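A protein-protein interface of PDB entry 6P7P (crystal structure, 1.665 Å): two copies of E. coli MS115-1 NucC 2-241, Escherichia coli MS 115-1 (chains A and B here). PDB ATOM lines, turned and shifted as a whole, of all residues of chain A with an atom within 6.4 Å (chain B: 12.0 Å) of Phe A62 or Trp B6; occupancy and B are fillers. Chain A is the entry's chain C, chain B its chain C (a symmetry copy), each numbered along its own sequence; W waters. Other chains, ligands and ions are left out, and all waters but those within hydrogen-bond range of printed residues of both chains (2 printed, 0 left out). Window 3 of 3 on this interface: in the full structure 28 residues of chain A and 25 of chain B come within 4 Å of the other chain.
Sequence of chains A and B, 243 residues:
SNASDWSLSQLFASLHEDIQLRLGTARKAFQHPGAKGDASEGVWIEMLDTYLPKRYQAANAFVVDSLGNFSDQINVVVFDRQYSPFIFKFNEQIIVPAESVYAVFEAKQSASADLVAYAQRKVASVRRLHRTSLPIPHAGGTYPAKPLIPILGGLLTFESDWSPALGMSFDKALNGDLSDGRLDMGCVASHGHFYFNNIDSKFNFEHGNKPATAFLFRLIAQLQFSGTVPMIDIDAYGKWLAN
The side-chain hydroxyl (OG) of Ser B7 lies close to the backbone NH (N) of Ser B9 (3.5 Å). O of Ile A94 sits at hydrogen-bond distance from N of Phe A62 (3.4 Å). OG of Ser B7 sits at hydrogen-bond distance from N of Gln B10. O of Phe A62 is in hydrogen-bond range of N of Val A96.
Printed residues of chain B that touch a printed residue of chain A: Trp B6, Ser B7, Leu B8 and Leu B11. Printed residues of chain A that touch a printed residue of chain B: Phe A62, Gly A68, Phe A70 and Ile A95. Among the printed residues, no Asp or Glu carboxylate lies within 4 Å of a Lys or Arg side-chain nitrogen of the other chain.
Trp B6 touches Phe A62. CA of Gly A68 touches CD2 of Leu B8, 3.99 Å away. CB of Trp B6 touches CD1 of Phe A70 (3.4 Å). Phe A70 touches Ser B7 (CZ to C, 3.8 Å). Phe A70 touches Leu B8 (CE1 to N, 3.6 Å). CD1 of Leu B11 touches CZ of Phe A70, at 3.9 Å. Ile A95 touches Trp B6 (CD1 to CZ3, 3.8 Å). CD1 of Leu B11 touches CD1 of Ile A95, at 3.6 Å.
Of chain B, only Trp B6 (3.6 Å) comes within 4 Å of Phe A62. Of chain A, only Phe A62 (3.6 Å), Phe A70 (3.4 Å) and Ile A95 (3.8 Å) come within 4 Å of Trp B6. No residue of chain B comes within 4 Å of Asn A60. Ala A61 touches none of the printed residues of chain B. No residue of chain B comes within 4 Å of Val A64. Phe A70 touches four residues of chain B. No residue of chain B comes within 4 Å of Ser A71. Gln A73 touches none of the printed residues of chain B. No residue of chain B comes within 4 Å of Ile A74. Ile A94 touches none of the printed residues of chain B. No residue of chain B comes within 4 Å of Val A96. Printed residues of chain A within 4 Å of Leu B11: Phe A70 (3.9 Å) and Ile A95 (3.6 Å). Of the printed residues of chain A, Leu B8 touches Gly A68 and Phe A70. Printed residues of chain A within 4 Å of Ser B7: Phe A70 (3.8 Å). Of the printed residues of chain B, Gly A68 touches Leu B8 (3.99 Å). The nearest residue of chain B that does not touch Phe A62 is Leu B11 (7.6 Å). The nearest printed residue of chain A that does not touch Ser B7 is Gly A68 (5.7 Å).
Water W2 lies within hydrogen-bond range of the backbone carbonyl oxygen (O) of Gly A68 (2.8 Å) and the backbone NH (N) of Leu B8 (2.9 Å). Water W1 lies within hydrogen-bond range of the backbone carbonyl oxygen (O) of Gly A68 and the backbone carbonyl oxygen (O) of Trp B6.
No position is printed for both chains.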
ATOM      1  N   ASN A  60      10.523  -4.931 -16.870  1.00  0.00           N
ATOM      2  CA  ASN A  60      11.358  -3.949 -17.547  1.00  0.00           C
ATOM      3  C   ASN A  60      10.785  -3.657 -18.930  1.00  0.00           C
ATOM      4  O   ASN A  60      10.422  -4.583 -19.653  1.00  0.00           O
ATOM      5  CB  ASN A  60      12.778  -4.523 -17.650  1.00  0.00           C
ATOM      6  CG  ASN A  60      13.724  -3.673 -18.457  1.00  0.00           C
ATOM      7  OD1 ASN A  60      13.462  -3.349 -19.618  1.00  0.00           O
ATOM      8  ND2 ASN A  60      14.860  -3.320 -17.847  1.00  0.00           N
ATOM      9  N   ALA A  61      10.726  -2.377 -19.327  1.00  0.00           N
ATOM     10  CA  ALA A  61      10.175  -2.053 -20.639  1.00  0.00           C
ATOM     11  C   ALA A  61      10.538  -0.645 -21.069  1.00  0.00           C
ATOM     12  O   ALA A  61      11.006   0.171 -20.280  1.00  0.00           O
ATOM     13  CB  ALA A  61       8.652  -2.184 -20.644  1.00  0.00           C
ATOM     14  N   PHE A  62      10.302  -0.372 -22.349  1.00  0.00           N
ATOM     15  CA  PHE A  62      10.200   0.966 -22.898  1.00  0.00           C
ATOM     16  C   PHE A  62       8.727   1.306 -23.046  1.00  0.00           C
ATOM     17  O   PHE A  62       7.888   0.428 -23.283  1.00  0.00           O
ATOM     18  CB  PHE A  62      10.893   1.067 -24.272  1.00  0.00           C
ATOM     19  CG  PHE A  62      12.398   0.906 -24.217  1.00  0.00           C
ATOM     20  CD1 PHE A  62      12.966  -0.352 -24.325  1.00  0.00           C
ATOM     21  CD2 PHE A  62      13.242   2.007 -24.056  1.00  0.00           C
ATOM     22  CE1 PHE A  62      14.342  -0.506 -24.256  1.00  0.00           C
ATOM     23  CE2 PHE A  62      14.613   1.844 -24.007  1.00  0.00           C
ATOM     24  CZ  PHE A  62      15.155   0.587 -24.079  1.00  0.00           C
ATOM     25  N   VAL A  63       8.415   2.591 -22.874  1.00  0.00           N
ATOM     26  CA  VAL A  63       7.066   3.113 -23.029  1.00  0.00           C
ATOM     27  C   VAL A  63       7.057   4.004 -24.259  1.00  0.00           C
ATOM     28  O   VAL A  63       7.999   4.753 -24.493  1.00  0.00           O
ATOM     29  CB  VAL A  63       6.620   3.905 -21.785  1.00  0.00           C
ATOM     30  CG1 VAL A  63       5.125   4.294 -21.909  1.00  0.00           C
ATOM     31  CG2 VAL A  63       6.871   3.111 -20.487  1.00  0.00           C
ATOM     32  N   VAL A  64       5.993   3.928 -25.049  1.00  0.00           N
ATOM     33  CA  VAL A  64       5.858   4.743 -26.252  1.00  0.00           C
ATOM     34  C   VAL A  64       4.450   5.324 -26.278  1.00  0.00           C
ATOM     35  O   VAL A  64       3.525   4.759 -25.684  1.00  0.00           O
ATOM     36  CB  VAL A  64       6.143   3.897 -27.516  1.00  0.00           C
ATOM     37  CG1 VAL A  64       5.089   2.820 -27.646  1.00  0.00           C
ATOM     38  CG2 VAL A  64       6.224   4.747 -28.755  1.00  0.00           C
ATOM     39  N   GLY A  68       4.557   9.041 -31.192  1.00  0.00           N
ATOM     40  CA  GLY A  68       5.832   8.484 -31.598  1.00  0.00           C
ATOM     41  C   GLY A  68       6.973   8.780 -30.669  1.00  0.00           C
ATOM     42  O   GLY A  68       8.130   8.551 -31.036  1.00  0.00           O
ATOM     43  N   PHE A  70       9.180   8.183 -27.163  1.00  0.00           N
ATOM     44  CA  PHE A  70       9.569   7.046 -26.352  1.00  0.00           C
ATOM     45  C   PHE A  70      10.155   7.509 -25.020  1.00  0.00           C
ATOM     46  O   PHE A  70      10.854   8.530 -24.941  1.00  0.00           O
ATOM     47  CB  PHE A  70      10.621   6.205 -27.075  1.00  0.00           C
ATOM     48  CG  PHE A  70      10.087   5.383 -28.234  1.00  0.00           C
ATOM     49  CD1 PHE A  70       9.702   5.985 -29.430  1.00  0.00           C
ATOM     50  CD2 PHE A  70      10.025   4.002 -28.135  1.00  0.00           C
ATOM     51  CE1 PHE A  70       9.239   5.225 -30.492  1.00  0.00           C
ATOM     52  CE2 PHE A  70       9.582   3.244 -29.202  1.00  0.00           C
ATOM     53  CZ  PHE A  70       9.187   3.851 -30.365  1.00  0.00           C
ATOM     54  N   SER A  71       9.893   6.727 -23.974  1.00  0.00           N
ATOM     55  CA  SER A  71      10.573   6.910 -22.705  1.00  0.00           C
ATOM     56  C   SER A  71      12.000   6.393 -22.785  1.00  0.00           C
ATOM     57  O   SER A  71      12.414   5.762 -23.759  1.00  0.00           O
ATOM     58  CB  SER A  71       9.834   6.161 -21.592  1.00  0.00           C
ATOM     59  OG  SER A  71      10.020   4.742 -21.680  1.00  0.00           O
ATOM     60  N   ASP A  72      12.759   6.652 -21.715  1.00  0.00           N
ATOM     61  CA  ASP A  72      13.998   5.928 -21.487  1.00  0.00           C
ATOM     62  C   ASP A  72      13.681   4.477 -21.102  1.00  0.00           C
ATOM     63  O   ASP A  72      12.519   4.095 -20.905  1.00  0.00           O
ATOM     64  CB  ASP A  72      14.817   6.623 -20.391  1.00  0.00           C
ATOM     65  CG  ASP A  72      15.016   8.113 -20.652  1.00  0.00           C
ATOM     66  OD1 ASP A  72      15.092   8.499 -21.830  1.00  0.00           O
ATOM     67  OD2 ASP A  72      15.091   8.891 -19.673  1.00  0.00           O
ATOM     68  N   GLN A  73      14.709   3.643 -21.003  1.00  0.00           N
ATOM     69  CA  GLN A  73      14.494   2.279 -20.523  1.00  0.00           C
ATOM     70  C   GLN A  73      14.080   2.344 -19.059  1.00  0.00           C
ATOM     71  O   GLN A  73      14.765   2.971 -18.243  1.00  0.00           O
ATOM     72  CB  GLN A  73      15.752   1.420 -20.677  1.00  0.00           C
ATOM     73  CG  GLN A  73      15.462  -0.063 -20.434  1.00  0.00           C
ATOM     74  CD  GLN A  73      16.628  -0.987 -20.737  1.00  0.00           C
ATOM     75  OE1 GLN A  73      17.778  -0.690 -20.407  1.00  0.00           O
ATOM     76  NE2 GLN A  73      16.333  -2.130 -21.364  1.00  0.00           N
ATOM     77  N   ILE A  74      12.957   1.728 -18.728  1.00  0.00           N
ATOM     78  CA  ILE A  74      12.421   1.771 -17.374  1.00  0.00           C
ATOM     79  C   ILE A  74      12.658   0.421 -16.723  1.00  0.00           C
ATOM     80  O   ILE A  74      12.184  -0.614 -17.220  1.00  0.00           O
ATOM     81  CB  ILE A  74      10.929   2.130 -17.358  1.00  0.00           C
ATOM     82  CG1 ILE A  74      10.642   3.402 -18.147  1.00  0.00           C
ATOM     83  CG2 ILE A  74      10.431   2.264 -15.926  1.00  0.00           C
ATOM     84  CD1 ILE A  74      11.423   4.630 -17.781  1.00  0.00           C
ATOM     85  N   VAL A  77       8.360  -1.265 -14.649  1.00  0.00           N
ATOM     86  CA  VAL A  77       7.101  -0.677 -15.061  1.00  0.00           C
ATOM     87  C   VAL A  77       5.995  -1.561 -14.519  1.00  0.00           C
ATOM     88  O   VAL A  77       6.048  -2.791 -14.684  1.00  0.00           O
ATOM     89  CB  VAL A  77       6.988  -0.584 -16.591  1.00  0.00           C
ATOM     90  CG1 VAL A  77       5.678   0.091 -16.973  1.00  0.00           C
ATOM     91  CG2 VAL A  77       8.161   0.150 -17.206  1.00  0.00           C
ATOM     92  N   GLN A  93      11.542  -9.026 -24.801  1.00  0.00           N
ATOM     93  CA  GLN A  93      11.628  -7.577 -24.750  1.00  0.00           C
ATOM     94  C   GLN A  93      10.316  -6.953 -25.193  1.00  0.00           C
ATOM     95  O   GLN A  93       9.758  -7.333 -26.232  1.00  0.00           O
ATOM     96  CB  GLN A  93      12.772  -7.104 -25.620  1.00  0.00           C
ATOM     97  CG  GLN A  93      14.078  -7.673 -25.099  1.00  0.00           C
ATOM     98  CD  GLN A  93      15.202  -7.432 -26.032  1.00  0.00           C
ATOM     99  OE1 GLN A  93      15.691  -8.357 -26.671  1.00  0.00           O
ATOM    100  NE2 GLN A  93      15.646  -6.187 -26.108  1.00  0.00           N
ATOM    101  N   ILE A  94       9.839  -5.979 -24.416  1.00  0.00           N
ATOM    102  CA  ILE A  94       8.518  -5.398 -24.629  1.00  0.00           C
ATOM    103  C   ILE A  94       8.556  -3.875 -24.688  1.00  0.00           C
ATOM    104  O   ILE A  94       9.355  -3.212 -24.016  1.00  0.00           O
ATOM    105  CB  ILE A  94       7.532  -5.854 -23.535  1.00  0.00           C
ATOM    106  CG1 ILE A  94       8.100  -5.586 -22.145  1.00  0.00           C
ATOM    107  CG2 ILE A  94       7.218  -7.330 -23.721  1.00  0.00           C
ATOM    108  CD1 ILE A  94       7.069  -5.680 -21.045  1.00  0.00           C
ATOM    109  N   ILE A  95       7.668  -3.329 -25.513  1.00  0.00           N
ATOM    110  CA  ILE A  95       7.389  -1.900 -25.593  1.00  0.00           C
ATOM    111  C   ILE A  95       5.908  -1.735 -25.334  1.00  0.00           C
ATOM    112  O   ILE A  95       5.085  -2.361 -26.013  1.00  0.00           O
ATOM    113  CB  ILE A  95       7.796  -1.313 -26.954  1.00  0.00           C
ATOM    114  CG1 ILE A  95       9.289  -1.611 -27.183  1.00  0.00           C
ATOM    115  CG2 ILE A  95       7.518   0.196 -27.003  1.00  0.00           C
ATOM    116  CD1 ILE A  95       9.813  -1.184 -28.517  1.00  0.00           C
ATOM    117  N   VAL A  96       5.568  -0.966 -24.307  1.00  0.00           N
ATOM    118  CA  VAL A  96       4.179  -0.844 -23.883  1.00  0.00           C
ATOM    119  C   VAL A  96       3.642   0.537 -24.234  1.00  0.00           C
ATOM    120  O   VAL A  96       4.398   1.519 -24.253  1.00  0.00           O
ATOM    121  CB  VAL A  96       4.017  -1.118 -22.368  1.00  0.00           C
ATOM    122  CG1 VAL A  96       4.447  -2.529 -22.031  1.00  0.00           C
ATOM    123  CG2 VAL A  96       4.775  -0.088 -21.535  1.00  0.00           C
ATOM    124  N   PRO A  97       2.340   0.672 -24.495  1.00  0.00           N
ATOM    125  CA  PRO A  97       1.778   1.999 -24.735  1.00  0.00           C
ATOM    126  C   PRO A  97       1.644   2.777 -23.440  1.00  0.00           C
ATOM    127  O   PRO A  97       1.403   2.212 -22.367  1.00  0.00           O
ATOM    128  CB  PRO A  97       0.409   1.679 -25.342  1.00  0.00           C
ATOM    129  CG  PRO A  97       0.024   0.400 -24.663  1.00  0.00           C
ATOM    130  CD  PRO A  97       1.303  -0.374 -24.563  1.00  0.00           C
ATOM    131  N   SER B   1      26.516   1.532 -36.842  1.00  0.00           N
ATOM    132  CA  SER B   1      26.812   2.865 -36.233  1.00  0.00           C
ATOM    133  C   SER B   1      26.188   2.908 -34.845  1.00  0.00           C
ATOM    134  O   SER B   1      25.453   1.993 -34.453  1.00  0.00           O
ATOM    135  CB  SER B   1      26.289   4.008 -37.107  1.00  0.00           C
ATOM    136  OG  SER B   1      25.007   4.437 -36.698  1.00  0.00           O
ATOM    137  N   ASN B   2      26.493   3.965 -34.096  1.00  0.00           N
ATOM    138  CA  ASN B   2      26.003   4.113 -32.733  1.00  0.00           C
ATOM    139  C   ASN B   2      24.766   4.998 -32.636  1.00  0.00           C
ATOM    140  O   ASN B   2      24.316   5.298 -31.526  1.00  0.00           O
ATOM    141  CB  ASN B   2      27.116   4.671 -31.835  1.00  0.00           C
ATOM    142  CG  ASN B   2      28.306   3.741 -31.744  1.00  0.00           C
ATOM    143  OD1 ASN B   2      28.153   2.516 -31.770  1.00  0.00           O
ATOM    144  ND2 ASN B   2      29.504   4.316 -31.639  1.00  0.00           N
ATOM    145  N   ALA B   3      24.198   5.410 -33.769  1.00  0.00           N
ATOM    146  CA  ALA B   3      23.013   6.258 -33.745  1.00  0.00           C
ATOM    147  C   ALA B   3      21.842   5.524 -33.106  1.00  0.00           C
ATOM    148  O   ALA B   3      21.679   4.316 -33.281  1.00  0.00           O
ATOM    149  CB  ALA B   3      22.640   6.665 -35.167  1.00  0.00           C
ATOM    150  N   SER B   4      21.031   6.261 -32.350  1.00  0.00           N
ATOM    151  CA  SER B   4      19.828   5.703 -31.749  1.00  0.00           C
ATOM    152  C   SER B   4      18.715   6.724 -31.930  1.00  0.00           C
ATOM    153  O   SER B   4      18.769   7.816 -31.360  1.00  0.00           O
ATOM    154  CB  SER B   4      20.037   5.356 -30.273  1.00  0.00           C
ATOM    155  OG  SER B   4      20.596   6.427 -29.540  1.00  0.00           O
ATOM    156  N   ASP B   5      17.720   6.375 -32.739  1.00  0.00           N
ATOM    157  CA  ASP B   5      16.538   7.230 -32.915  1.00  0.00           C
ATOM    158  C   ASP B   5      15.332   6.311 -33.040  1.00  0.00           C
ATOM    159  O   ASP B   5      15.070   5.738 -34.106  1.00  0.00           O
ATOM    160  CB  ASP B   5      16.703   8.144 -34.122  1.00  0.00           C
ATOM    161  CG  ASP B   5      17.718   9.245 -33.880  1.00  0.00           C
ATOM    162  OD1 ASP B   5      17.474  10.141 -33.035  1.00  0.00           O
ATOM    163  OD2 ASP B   5      18.782   9.203 -34.505  1.00  0.00           O
ATOM    164  N   TRP B   6      14.619   6.141 -31.921  1.00  0.00           N
ATOM    165  CA  TRP B   6      13.465   5.264 -31.876  1.00  0.00           C
ATOM    166  C   TRP B   6      12.400   5.663 -32.898  1.00  0.00           C
ATOM    167  O   TRP B   6      12.145   6.853 -33.134  1.00  0.00           O
ATOM    168  CB  TRP B   6      12.846   5.310 -30.496  1.00  0.00           C
ATOM    169  CG  TRP B   6      13.484   4.541 -29.418  1.00  0.00           C
ATOM    170  CD1 TRP B   6      14.205   5.043 -28.393  1.00  0.00           C
ATOM    171  CD2 TRP B   6      13.405   3.134 -29.210  1.00  0.00           C
ATOM    172  NE1 TRP B   6      14.607   4.027 -27.556  1.00  0.00           N
ATOM    173  CE2 TRP B   6      14.094   2.845 -28.021  1.00  0.00           C
ATOM    174  CE3 TRP B   6      12.803   2.089 -29.908  1.00  0.00           C
ATOM    175  CZ2 TRP B   6      14.220   1.544 -27.529  1.00  0.00           C
ATOM    176  CZ3 TRP B   6      12.899   0.813 -29.407  1.00  0.00           C
ATOM    177  CH2 TRP B   6      13.603   0.548 -28.225  1.00  0.00           C
ATOM    178  N   SER B   7      11.778   4.656 -33.498  1.00  0.00           N
ATOM    179  CA  SER B   7      10.730   4.842 -34.498  1.00  0.00           C
ATOM    180  C   SER B   7       9.537   3.950 -34.183  1.00  0.00           C
ATOM    181  O   SER B   7       9.655   2.727 -34.200  1.00  0.00           O
ATOM    182  CB  SER B   7      11.278   4.516 -35.885  1.00  0.00           C
ATOM    183  OG  SER B   7      10.233   4.501 -36.856  1.00  0.00           O
ATOM    184  N   LEU B   8       8.373   4.568 -33.974  1.00  0.00           N
ATOM    185  CA  LEU B   8       7.149   3.807 -33.793  1.00  0.00           C
ATOM    186  C   LEU B   8       6.735   3.115 -35.085  1.00  0.00           C
ATOM    187  O   LEU B   8       6.323   1.951 -35.067  1.00  0.00           O
ATOM    188  CB  LEU B   8       6.053   4.742 -33.280  1.00  0.00           C
ATOM    189  CG  LEU B   8       4.680   4.138 -33.084  1.00  0.00           C
ATOM    190  CD1 LEU B   8       4.678   2.951 -32.132  1.00  0.00           C
ATOM    191  CD2 LEU B   8       3.738   5.226 -32.540  1.00  0.00           C
ATOM    192  N   SER B   9       6.871   3.803 -36.221  1.00  0.00           N
ATOM    193  CA  SER B   9       6.543   3.183 -37.496  1.00  0.00           C
ATOM    194  C   SER B   9       7.337   1.905 -37.719  1.00  0.00           C
ATOM    195  O   SER B   9       6.804   0.914 -38.234  1.00  0.00           O
ATOM    196  CB  SER B   9       6.798   4.168 -38.634  1.00  0.00           C
ATOM    197  OG  SER B   9       5.729   5.083 -38.749  1.00  0.00           O
ATOM    198  N   GLN B  10       8.621   1.903 -37.344  1.00  0.00           N
ATOM    199  CA  GLN B  10       9.441   0.711 -37.540  1.00  0.00           C
ATOM    200  C   GLN B  10       8.926  -0.464 -36.719  1.00  0.00           C
ATOM    201  O   GLN B  10       9.008  -1.619 -37.156  1.00  0.00           O
ATOM    202  CB  GLN B  10      10.899   0.999 -37.179  1.00  0.00           C
ATOM    203  CG  GLN B  10      11.823  -0.229 -37.346  1.00  0.00           C
ATOM    204  CD  GLN B  10      11.913  -0.710 -38.784  1.00  0.00           C
ATOM    205  OE1 GLN B  10      12.297   0.053 -39.689  1.00  0.00           O
ATOM    206  NE2 GLN B  10      11.552  -1.990 -39.020  1.00  0.00           N
ATOM    207  N   LEU B  11       8.425  -0.207 -35.515  1.00  0.00           N
ATOM    208  CA  LEU B  11       7.869  -1.297 -34.722  1.00  0.00           C
ATOM    209  C   LEU B  11       6.726  -1.974 -35.468  1.00  0.00           C
ATOM    210  O   LEU B  11       6.652  -3.207 -35.537  1.00  0.00           O
ATOM    211  CB  LEU B  11       7.377  -0.768 -33.374  1.00  0.00           C
ATOM    212  CG  LEU B  11       8.418  -0.049 -32.522  1.00  0.00           C
ATOM    213  CD1 LEU B  11       7.863   0.311 -31.169  1.00  0.00           C
ATOM    214  CD2 LEU B  11       9.634  -0.930 -32.403  1.00  0.00           C
ATOM    215  N   PHE B  12       5.854  -1.176 -36.067  1.00  0.00           N
ATOM    216  CA  PHE B  12       4.697  -1.723 -36.771  1.00  0.00           C
ATOM    217  C   PHE B  12       5.098  -2.423 -38.056  1.00  0.00           C
ATOM    218  O   PHE B  12       4.471  -3.421 -38.430  1.00  0.00           O
ATOM    219  CB  PHE B  12       3.692  -0.602 -37.031  1.00  0.00           C
ATOM    220  CG  PHE B  12       3.127  -0.015 -35.761  1.00  0.00           C
ATOM    221  CD1 PHE B  12       3.082  -0.776 -34.594  1.00  0.00           C
ATOM    222  CD2 PHE B  12       2.636   1.263 -35.731  1.00  0.00           C
ATOM    223  CE1 PHE B  12       2.582  -0.254 -33.439  1.00  0.00           C
ATOM    224  CE2 PHE B  12       2.119   1.785 -34.575  1.00  0.00           C
ATOM    225  CZ  PHE B  12       2.100   1.027 -33.429  1.00  0.00           C
ATOM    226  N   ALA B  13       6.145  -1.944 -38.720  1.00  0.00           N
ATOM    227  CA  ALA B  13       6.695  -2.646 -39.872  1.00  0.00           C
ATOM    228  C   ALA B  13       7.219  -4.015 -39.473  1.00  0.00           C
ATOM    229  O   ALA B  13       6.951  -5.016 -40.141  1.00  0.00           O
ATOM    230  CB  ALA B  13       7.813  -1.825 -40.506  1.00  0.00           C
ATOM    231  N   SER B  14       7.999  -4.072 -38.388  1.00  0.00           N
ATOM    232  CA  SER B  14       8.602  -5.330 -37.959  1.00  0.00           C
ATOM    233  C   SER B  14       7.551  -6.327 -37.475  1.00  0.00           C
ATOM    234  O   SER B  14       7.693  -7.534 -37.690  1.00  0.00           O
ATOM    235  CB  SER B  14       9.610  -5.020 -36.857  1.00  0.00           C
ATOM    236  OG  SER B  14      10.704  -4.307 -37.416  1.00  0.00           O
ATOM    237  N   LEU B  15       6.500  -5.835 -36.829  1.00  0.00           N
ATOM    238  CA  LEU B  15       5.401  -6.719 -36.447  1.00  0.00           C
ATOM    239  C   LEU B  15       4.795  -7.378 -37.679  1.00  0.00           C
ATOM    240  O   LEU B  15       4.620  -8.601 -37.727  1.00  0.00           O
ATOM    241  CB  LEU B  15       4.360  -5.913 -35.676  1.00  0.00           C
ATOM    242  CG  LEU B  15       3.301  -6.655 -34.854  1.00  0.00           C
ATOM    243  CD1 LEU B  15       2.647  -5.639 -33.921  1.00  0.00           C
ATOM    244  CD2 LEU B  15       2.270  -7.313 -35.773  1.00  0.00           C
ATOM    245  N   TYR B  51      -0.543 -10.096 -28.786  1.00  0.00           N
ATOM    246  CA  TYR B  51      -0.873  -8.674 -28.800  1.00  0.00           C
ATOM    247  C   TYR B  51      -2.264  -8.319 -28.299  1.00  0.00           C
ATOM    248  O   TYR B  51      -2.441  -7.187 -27.806  1.00  0.00           O
ATOM    249  CB  TYR B  51      -0.702  -8.125 -30.219  1.00  0.00           C
ATOM    250  CG  TYR B  51       0.773  -7.967 -30.576  1.00  0.00           C
ATOM    251  CD1 TYR B  51       1.497  -6.935 -30.045  1.00  0.00           C
ATOM    252  CD2 TYR B  51       1.437  -8.885 -31.399  1.00  0.00           C
ATOM    253  CE1 TYR B  51       2.840  -6.789 -30.322  1.00  0.00           C
ATOM    254  CE2 TYR B  51       2.789  -8.739 -31.681  1.00  0.00           C
ATOM    255  CZ  TYR B  51       3.477  -7.682 -31.142  1.00  0.00           C
ATOM    256  OH  TYR B  51       4.833  -7.499 -31.390  1.00  0.00           O
HETATM  257  O   HOH W   1      11.026   9.214 -31.050  1.00  0.00           O
HETATM  258  O   HOH W   2       8.442   7.426 -33.632  1.00  0.00           O
